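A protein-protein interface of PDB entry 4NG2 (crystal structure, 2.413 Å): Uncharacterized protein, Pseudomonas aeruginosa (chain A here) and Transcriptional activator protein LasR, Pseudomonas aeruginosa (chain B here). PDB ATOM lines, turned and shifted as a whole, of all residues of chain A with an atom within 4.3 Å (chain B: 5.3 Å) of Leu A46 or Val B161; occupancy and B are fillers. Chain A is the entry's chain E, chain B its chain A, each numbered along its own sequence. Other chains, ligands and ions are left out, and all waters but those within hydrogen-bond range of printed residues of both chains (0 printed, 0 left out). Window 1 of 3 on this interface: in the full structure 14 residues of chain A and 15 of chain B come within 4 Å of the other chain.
OG1 of Thr B164 lies within hydrogen-bond range of O of Leu A46. O of Ser B160 lies within hydrogen-bond range of N of Leu A46, 2.9 Å away.
The backbone carbonyl oxygen (O) of Leu A30 sits at hydrogen-bond distance from the backbone NH (N) of Trp A47 (3.0 Å).
Among the printed residues, pairs that only touch across the chains: Leu A45 with Ser B160 (3.3 Å), Trp A47 with Pro B163 (3.5 Å), Leu A45 with Glu B159 (3.6 Å), Leu A45 with Pro B163 (3.6 Å), Leu A46 with Leu B44 (3.8 Å), Trp A47 with Thr B164 (3.9 Å), Leu A46 with Val B161 (3.9 Å) and Tyr A27 with Leu B17 (3.99 Å).
Of chain B, only Leu B44 (3.8 Å), Ser B160 (2.9 Å), Val B161 (3.9 Å) and Thr B164 (2.6 Å) come within 4 Å of Leu A46. Of chain A, only Leu A46 comes within 4 Å of Val B161. Printed residues of chain B within 4 Å of Trp A47: Pro B163 and Thr B164. Of the printed residues of chain B, Leu A45 touches Glu B159 (3.6 Å), Ser B160 (3.3 Å) and Pro B163 (3.6 Å). Of the printed residues of chain B, Tyr A27 touches Leu B17 (3.99 Å). Phe B157 touches none of the printed residues of chain A. Leu B165 touches none of the printed residues of chain A. The nearest residue of chain B that does not touch Leu A46 is Pro B163 (4.2 Å). The nearest printed residue of chain A that does not touch Val B161 is Leu A45 (5.4 Å).
Hydrophobic or aromatic side chains of chain A within 4 Å of the printed part of chain B: Tyr A27, Leu A45, Leu A46 and Trp A47. Among the printed residues, no Asp or Glu carboxylate lies within 4 Å of a Lys or Arg side-chain nitrogen of the other chain.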
ATOM      1  N   TYR A  27     -13.785 -17.419   8.841  1.00  0.00           N
ATOM      2  CA  TYR A  27     -13.116 -18.110   9.965  1.00  0.00           C
ATOM      3  C   TYR A  27     -12.075 -17.199  10.627  1.00  0.00           C
ATOM      4  O   TYR A  27     -11.217 -17.667  11.375  1.00  0.00           O
ATOM      5  CB  TYR A  27     -12.445 -19.445   9.536  1.00  0.00           C
ATOM      6  CG  TYR A  27     -13.380 -20.412   8.846  1.00  0.00           C
ATOM      7  CD1 TYR A  27     -14.730 -20.436   9.166  1.00  0.00           C
ATOM      8  CD2 TYR A  27     -12.926 -21.274   7.851  1.00  0.00           C
ATOM      9  CE1 TYR A  27     -15.608 -21.290   8.540  1.00  0.00           C
ATOM     10  CE2 TYR A  27     -13.799 -22.141   7.205  1.00  0.00           C
ATOM     11  CZ  TYR A  27     -15.148 -22.145   7.556  1.00  0.00           C
ATOM     12  OH  TYR A  27     -16.058 -22.991   6.938  1.00  0.00           O
ATOM     13  N   LEU A  30     -12.538 -17.622  14.395  1.00  0.00           N
ATOM     14  CA  LEU A  30     -12.337 -18.967  14.914  1.00  0.00           C
ATOM     15  C   LEU A  30     -10.885 -19.399  14.913  1.00  0.00           C
ATOM     16  O   LEU A  30     -10.568 -20.491  15.385  1.00  0.00           O
ATOM     17  CB  LEU A  30     -13.161 -19.961  14.109  1.00  0.00           C
ATOM     18  CG  LEU A  30     -14.658 -19.649  14.121  1.00  0.00           C
ATOM     19  CD1 LEU A  30     -15.427 -20.544  13.147  1.00  0.00           C
ATOM     20  CD2 LEU A  30     -15.188 -19.791  15.546  1.00  0.00           C
ATOM     21  N   MET A  31      -9.999 -18.544  14.401  1.00  0.00           N
ATOM     22  CA  MET A  31      -8.555 -18.819  14.437  1.00  0.00           C
ATOM     23  C   MET A  31      -7.935 -18.512  15.816  1.00  0.00           C
ATOM     24  O   MET A  31      -8.329 -17.563  16.482  1.00  0.00           O
ATOM     25  CB  MET A  31      -7.822 -18.034  13.334  1.00  0.00           C
ATOM     26  CG  MET A  31      -8.176 -18.433  11.895  1.00  0.00           C
ATOM     27  SD  MET A  31      -7.611 -20.079  11.379  1.00  0.00           S
ATOM     28  CE  MET A  31      -5.825 -19.979  11.472  1.00  0.00           C
ATOM     29  N   LEU A  45      -4.040 -22.005  14.144  1.00  0.00           N
ATOM     30  CA  LEU A  45      -4.898 -23.187  14.188  1.00  0.00           C
ATOM     31  C   LEU A  45      -6.346 -22.770  14.107  1.00  0.00           C
ATOM     32  O   LEU A  45      -6.762 -21.884  14.836  1.00  0.00           O
ATOM     33  CB  LEU A  45      -4.676 -23.904  15.521  1.00  0.00           C
ATOM     34  CG  LEU A  45      -3.913 -25.222  15.652  1.00  0.00           C
ATOM     35  CD1 LEU A  45      -3.001 -25.482  14.483  1.00  0.00           C
ATOM     36  CD2 LEU A  45      -3.164 -25.298  17.006  1.00  0.00           C
ATOM     37  N   LEU A  46      -7.116 -23.398  13.227  1.00  0.00           N
ATOM     38  CA  LEU A  46      -8.544 -23.105  13.106  1.00  0.00           C
ATOM     39  C   LEU A  46      -9.344 -23.984  14.048  1.00  0.00           C
ATOM     40  O   LEU A  46      -9.178 -25.197  14.033  1.00  0.00           O
ATOM     41  CB  LEU A  46      -9.019 -23.367  11.684  1.00  0.00           C
ATOM     42  CG  LEU A  46     -10.501 -23.680  11.564  1.00  0.00           C
ATOM     43  CD1 LEU A  46     -11.293 -22.411  11.678  1.00  0.00           C
ATOM     44  CD2 LEU A  46     -10.775 -24.346  10.234  1.00  0.00           C
ATOM     45  N   TRP A  47     -10.208 -23.372  14.857  1.00  0.00           N
ATOM     46  CA  TRP A  47     -11.005 -24.091  15.858  1.00  0.00           C
ATOM     47  C   TRP A  47     -12.482 -23.859  15.594  1.00  0.00           C
ATOM     48  O   TRP A  47     -12.869 -22.775  15.170  1.00  0.00           O
ATOM     49  CB  TRP A  47     -10.663 -23.625  17.267  1.00  0.00           C
ATOM     50  CG  TRP A  47     -10.628 -24.721  18.273  1.00  0.00           C
ATOM     51  CD1 TRP A  47     -11.608 -25.053  19.177  1.00  0.00           C
ATOM     52  CD2 TRP A  47      -9.555 -25.634  18.496  1.00  0.00           C
ATOM     53  NE1 TRP A  47     -11.208 -26.121  19.932  1.00  0.00           N
ATOM     54  CE2 TRP A  47      -9.947 -26.493  19.542  1.00  0.00           C
ATOM     55  CE3 TRP A  47      -8.299 -25.814  17.909  1.00  0.00           C
ATOM     56  CZ2 TRP A  47      -9.128 -27.526  20.006  1.00  0.00           C
ATOM     57  CZ3 TRP A  47      -7.488 -26.832  18.373  1.00  0.00           C
ATOM     58  CH2 TRP A  47      -7.901 -27.673  19.409  1.00  0.00           C
ATOM     59  N   LEU B  17     -19.346 -24.622  11.315  1.00  0.00           N
ATOM     60  CA  LEU B  17     -18.776 -25.965  11.421  1.00  0.00           C
ATOM     61  C   LEU B  17     -19.441 -26.754  12.558  1.00  0.00           C
ATOM     62  O   LEU B  17     -19.691 -27.965  12.427  1.00  0.00           O
ATOM     63  CB  LEU B  17     -17.284 -25.869  11.714  1.00  0.00           C
ATOM     64  CG  LEU B  17     -16.463 -25.060  10.719  1.00  0.00           C
ATOM     65  CD1 LEU B  17     -15.210 -24.508  11.353  1.00  0.00           C
ATOM     66  CD2 LEU B  17     -16.139 -25.974   9.582  1.00  0.00           C
ATOM     67  N   LEU B  44     -14.594 -26.178   4.312  1.00  0.00           N
ATOM     68  CA  LEU B  44     -13.253 -26.134   4.891  1.00  0.00           C
ATOM     69  C   LEU B  44     -12.208 -25.905   3.800  1.00  0.00           C
ATOM     70  O   LEU B  44     -10.997 -25.948   4.052  1.00  0.00           O
ATOM     71  CB  LEU B  44     -12.959 -27.400   5.706  1.00  0.00           C
ATOM     72  CG  LEU B  44     -13.690 -27.398   7.056  1.00  0.00           C
ATOM     73  CD1 LEU B  44     -13.712 -28.765   7.694  1.00  0.00           C
ATOM     74  CD2 LEU B  44     -13.066 -26.408   7.996  1.00  0.00           C
ATOM     75  N   PHE B  46     -11.858 -27.696   1.011  1.00  0.00           N
ATOM     76  CA  PHE B  46     -11.470 -28.947   0.371  1.00  0.00           C
ATOM     77  C   PHE B  46     -12.518 -29.371  -0.666  1.00  0.00           C
ATOM     78  O   PHE B  46     -13.666 -29.641  -0.325  1.00  0.00           O
ATOM     79  CB  PHE B  46     -11.290 -30.044   1.410  1.00  0.00           C
ATOM     80  CG  PHE B  46     -10.127 -29.826   2.335  1.00  0.00           C
ATOM     81  CD1 PHE B  46     -10.257 -29.031   3.461  1.00  0.00           C
ATOM     82  CD2 PHE B  46      -8.910 -30.440   2.094  1.00  0.00           C
ATOM     83  CE1 PHE B  46      -9.192 -28.839   4.322  1.00  0.00           C
ATOM     84  CE2 PHE B  46      -7.840 -30.248   2.950  1.00  0.00           C
ATOM     85  CZ  PHE B  46      -7.984 -29.446   4.069  1.00  0.00           C
ATOM     86  N   PHE B 157      -1.486 -24.960   5.044  1.00  0.00           N
ATOM     87  CA  PHE B 157      -2.923 -24.863   5.187  1.00  0.00           C
ATOM     88  C   PHE B 157      -3.499 -26.038   5.980  1.00  0.00           C
ATOM     89  O   PHE B 157      -4.323 -25.843   6.874  1.00  0.00           O
ATOM     90  CB  PHE B 157      -3.602 -24.794   3.837  1.00  0.00           C
ATOM     91  CG  PHE B 157      -5.096 -24.854   3.920  1.00  0.00           C
ATOM     92  CD1 PHE B 157      -5.824 -23.735   4.278  1.00  0.00           C
ATOM     93  CD2 PHE B 157      -5.775 -26.033   3.651  1.00  0.00           C
ATOM     94  CE1 PHE B 157      -7.197 -23.792   4.355  1.00  0.00           C
ATOM     95  CE2 PHE B 157      -7.152 -26.085   3.727  1.00  0.00           C
ATOM     96  CZ  PHE B 157      -7.860 -24.964   4.070  1.00  0.00           C
ATOM     97  N   MET B 158      -3.058 -27.247   5.653  1.00  0.00           N
ATOM     98  CA  MET B 158      -3.593 -28.451   6.261  1.00  0.00           C
ATOM     99  C   MET B 158      -3.147 -28.605   7.696  1.00  0.00           C
ATOM    100  O   MET B 158      -3.775 -29.327   8.456  1.00  0.00           O
ATOM    101  CB  MET B 158      -3.208 -29.702   5.460  1.00  0.00           C
ATOM    102  CG  MET B 158      -4.002 -29.894   4.171  1.00  0.00           C
ATOM    103  SD  MET B 158      -3.680 -31.502   3.412  1.00  0.00           S
ATOM    104  CE  MET B 158      -2.109 -31.184   2.600  1.00  0.00           C
ATOM    105  N   GLU B 159      -2.067 -27.945   8.084  1.00  0.00           N
ATOM    106  CA  GLU B 159      -1.622 -28.068   9.465  1.00  0.00           C
ATOM    107  C   GLU B 159      -2.445 -27.155  10.378  1.00  0.00           C
ATOM    108  O   GLU B 159      -2.659 -27.473  11.553  1.00  0.00           O
ATOM    109  CB  GLU B 159      -0.131 -27.782   9.599  1.00  0.00           C
ATOM    110  CG  GLU B 159       0.511 -28.528  10.751  1.00  0.00           C
ATOM    111  CD  GLU B 159       0.595 -30.024  10.497  1.00  0.00           C
ATOM    112  OE1 GLU B 159       1.165 -30.407   9.454  1.00  0.00           O
ATOM    113  OE2 GLU B 159       0.097 -30.814  11.337  1.00  0.00           O
ATOM    114  N   SER B 160      -2.914 -26.034   9.825  1.00  0.00           N
ATOM    115  CA  SER B 160      -3.745 -25.091  10.558  1.00  0.00           C
ATOM    116  C   SER B 160      -5.123 -25.642  10.810  1.00  0.00           C
ATOM    117  O   SER B 160      -5.666 -25.464  11.898  1.00  0.00           O
ATOM    118  CB  SER B 160      -3.892 -23.782   9.796  1.00  0.00           C
ATOM    119  OG  SER B 160      -2.620 -23.302   9.440  1.00  0.00           O
ATOM    120  N   VAL B 161      -5.693 -26.293   9.797  1.00  0.00           N
ATOM    121  CA  VAL B 161      -7.056 -26.798   9.891  1.00  0.00           C
ATOM    122  C   VAL B 161      -7.092 -28.217  10.407  1.00  0.00           C
ATOM    123  O   VAL B 161      -8.166 -28.781  10.602  1.00  0.00           O
ATOM    124  CB  VAL B 161      -7.814 -26.747   8.541  1.00  0.00           C
ATOM    125  CG1 VAL B 161      -7.792 -25.329   7.962  1.00  0.00           C
ATOM    126  CG2 VAL B 161      -7.242 -27.761   7.562  1.00  0.00           C
ATOM    127  N   LEU B 162      -5.928 -28.812  10.626  1.00  0.00           N
ATOM    128  CA  LEU B 162      -5.896 -30.208  11.061  1.00  0.00           C
ATOM    129  C   LEU B 162      -6.716 -30.510  12.322  1.00  0.00           C
ATOM    130  O   LEU B 162      -7.304 -31.582  12.408  1.00  0.00           O
ATOM    131  CB  LEU B 162      -4.467 -30.727  11.212  1.00  0.00           C
ATOM    132  CG  LEU B 162      -4.418 -32.216  11.572  1.00  0.00           C
ATOM    133  CD1 LEU B 162      -5.170 -33.031  10.552  1.00  0.00           C
ATOM    134  CD2 LEU B 162      -2.970 -32.676  11.665  1.00  0.00           C
ATOM    135  N   PRO B 163      -6.727 -29.601  13.317  1.00  0.00           N
ATOM    136  CA  PRO B 163      -7.540 -29.820  14.529  1.00  0.00           C
ATOM    137  C   PRO B 163      -9.058 -29.880  14.260  1.00  0.00           C
ATOM    138  O   PRO B 163      -9.791 -30.691  14.840  1.00  0.00           O
ATOM    139  CB  PRO B 163      -7.203 -28.601  15.392  1.00  0.00           C
ATOM    140  CG  PRO B 163      -5.794 -28.266  15.006  1.00  0.00           C
ATOM    141  CD  PRO B 163      -5.692 -28.563  13.530  1.00  0.00           C
ATOM    142  N   THR B 164      -9.531 -29.010  13.384  1.00  0.00           N
ATOM    143  CA  THR B 164     -10.922 -29.024  13.017  1.00  0.00           C
ATOM    144  C   THR B 164     -11.228 -30.289  12.241  1.00  0.00           C
ATOM    145  O   THR B 164     -12.305 -30.850  12.363  1.00  0.00           O
ATOM    146  CB  THR B 164     -11.247 -27.817  12.164  1.00  0.00           C
ATOM    147  OG1 THR B 164     -11.124 -26.639  12.974  1.00  0.00           O
ATOM    148  CG2 THR B 164     -12.652 -27.923  11.606  1.00  0.00           C
ATOM    149  N   LEU B 165     -10.265 -30.735  11.442  1.00  0.00           N
ATOM    150  CA  LEU B 165     -10.413 -31.951  10.636  1.00  0.00           C
ATOM    151  C   LEU B 165     -10.411 -33.191  11.512  1.00  0.00           C
ATOM    152  O   LEU B 165     -11.066 -34.183  11.213  1.00  0.00           O
ATOM    153  CB  LEU B 165      -9.261 -32.078   9.642  1.00  0.00           C
ATOM    154  CG  LEU B 165      -9.256 -31.155   8.443  1.00  0.00           C
ATOM    155  CD1 LEU B 165      -8.261 -31.699   7.435  1.00  0.00           C
ATOM    156  CD2 LEU B 165     -10.651 -31.122   7.860  1.00  0.00           C
ATOM    157  N   TRP B 166      -9.650 -33.149  12.591  1.00  0.00           N
ATOM    158  CA  TRP B 166      -9.613 -34.313  13.438  1.00  0.00           C
ATOM    159  C   TRP B 166     -10.941 -34.463  14.155  1.00  0.00           C
ATOM    160  O   TRP B 166     -11.363 -35.572  14.448  1.00  0.00           O
ATOM    161  CB  TRP B 166      -8.397 -34.300  14.365  1.00  0.00           C
ATOM    162  CG  TRP B 166      -8.650 -34.022  15.788  1.00  0.00           C
ATOM    163  CD1 TRP B 166      -8.728 -32.795  16.388  1.00  0.00           C
ATOM    164  CD2 TRP B 166      -8.798 -34.984  16.824  1.00  0.00           C
ATOM    165  NE1 TRP B 166      -8.931 -32.938  17.741  1.00  0.00           N
ATOM    166  CE2 TRP B 166      -8.977 -34.274  18.035  1.00  0.00           C
ATOM    167  CE3 TRP B 166      -8.801 -36.364  16.849  1.00  0.00           C
ATOM    168  CZ2 TRP B 166      -9.164 -34.910  19.257  1.00  0.00           C
ATOM    169  CZ3 TRP B 166      -8.991 -36.996  18.062  1.00  0.00           C
ATOM    170  CH2 TRP B 166      -9.171 -36.269  19.251  1.00  0.00           C
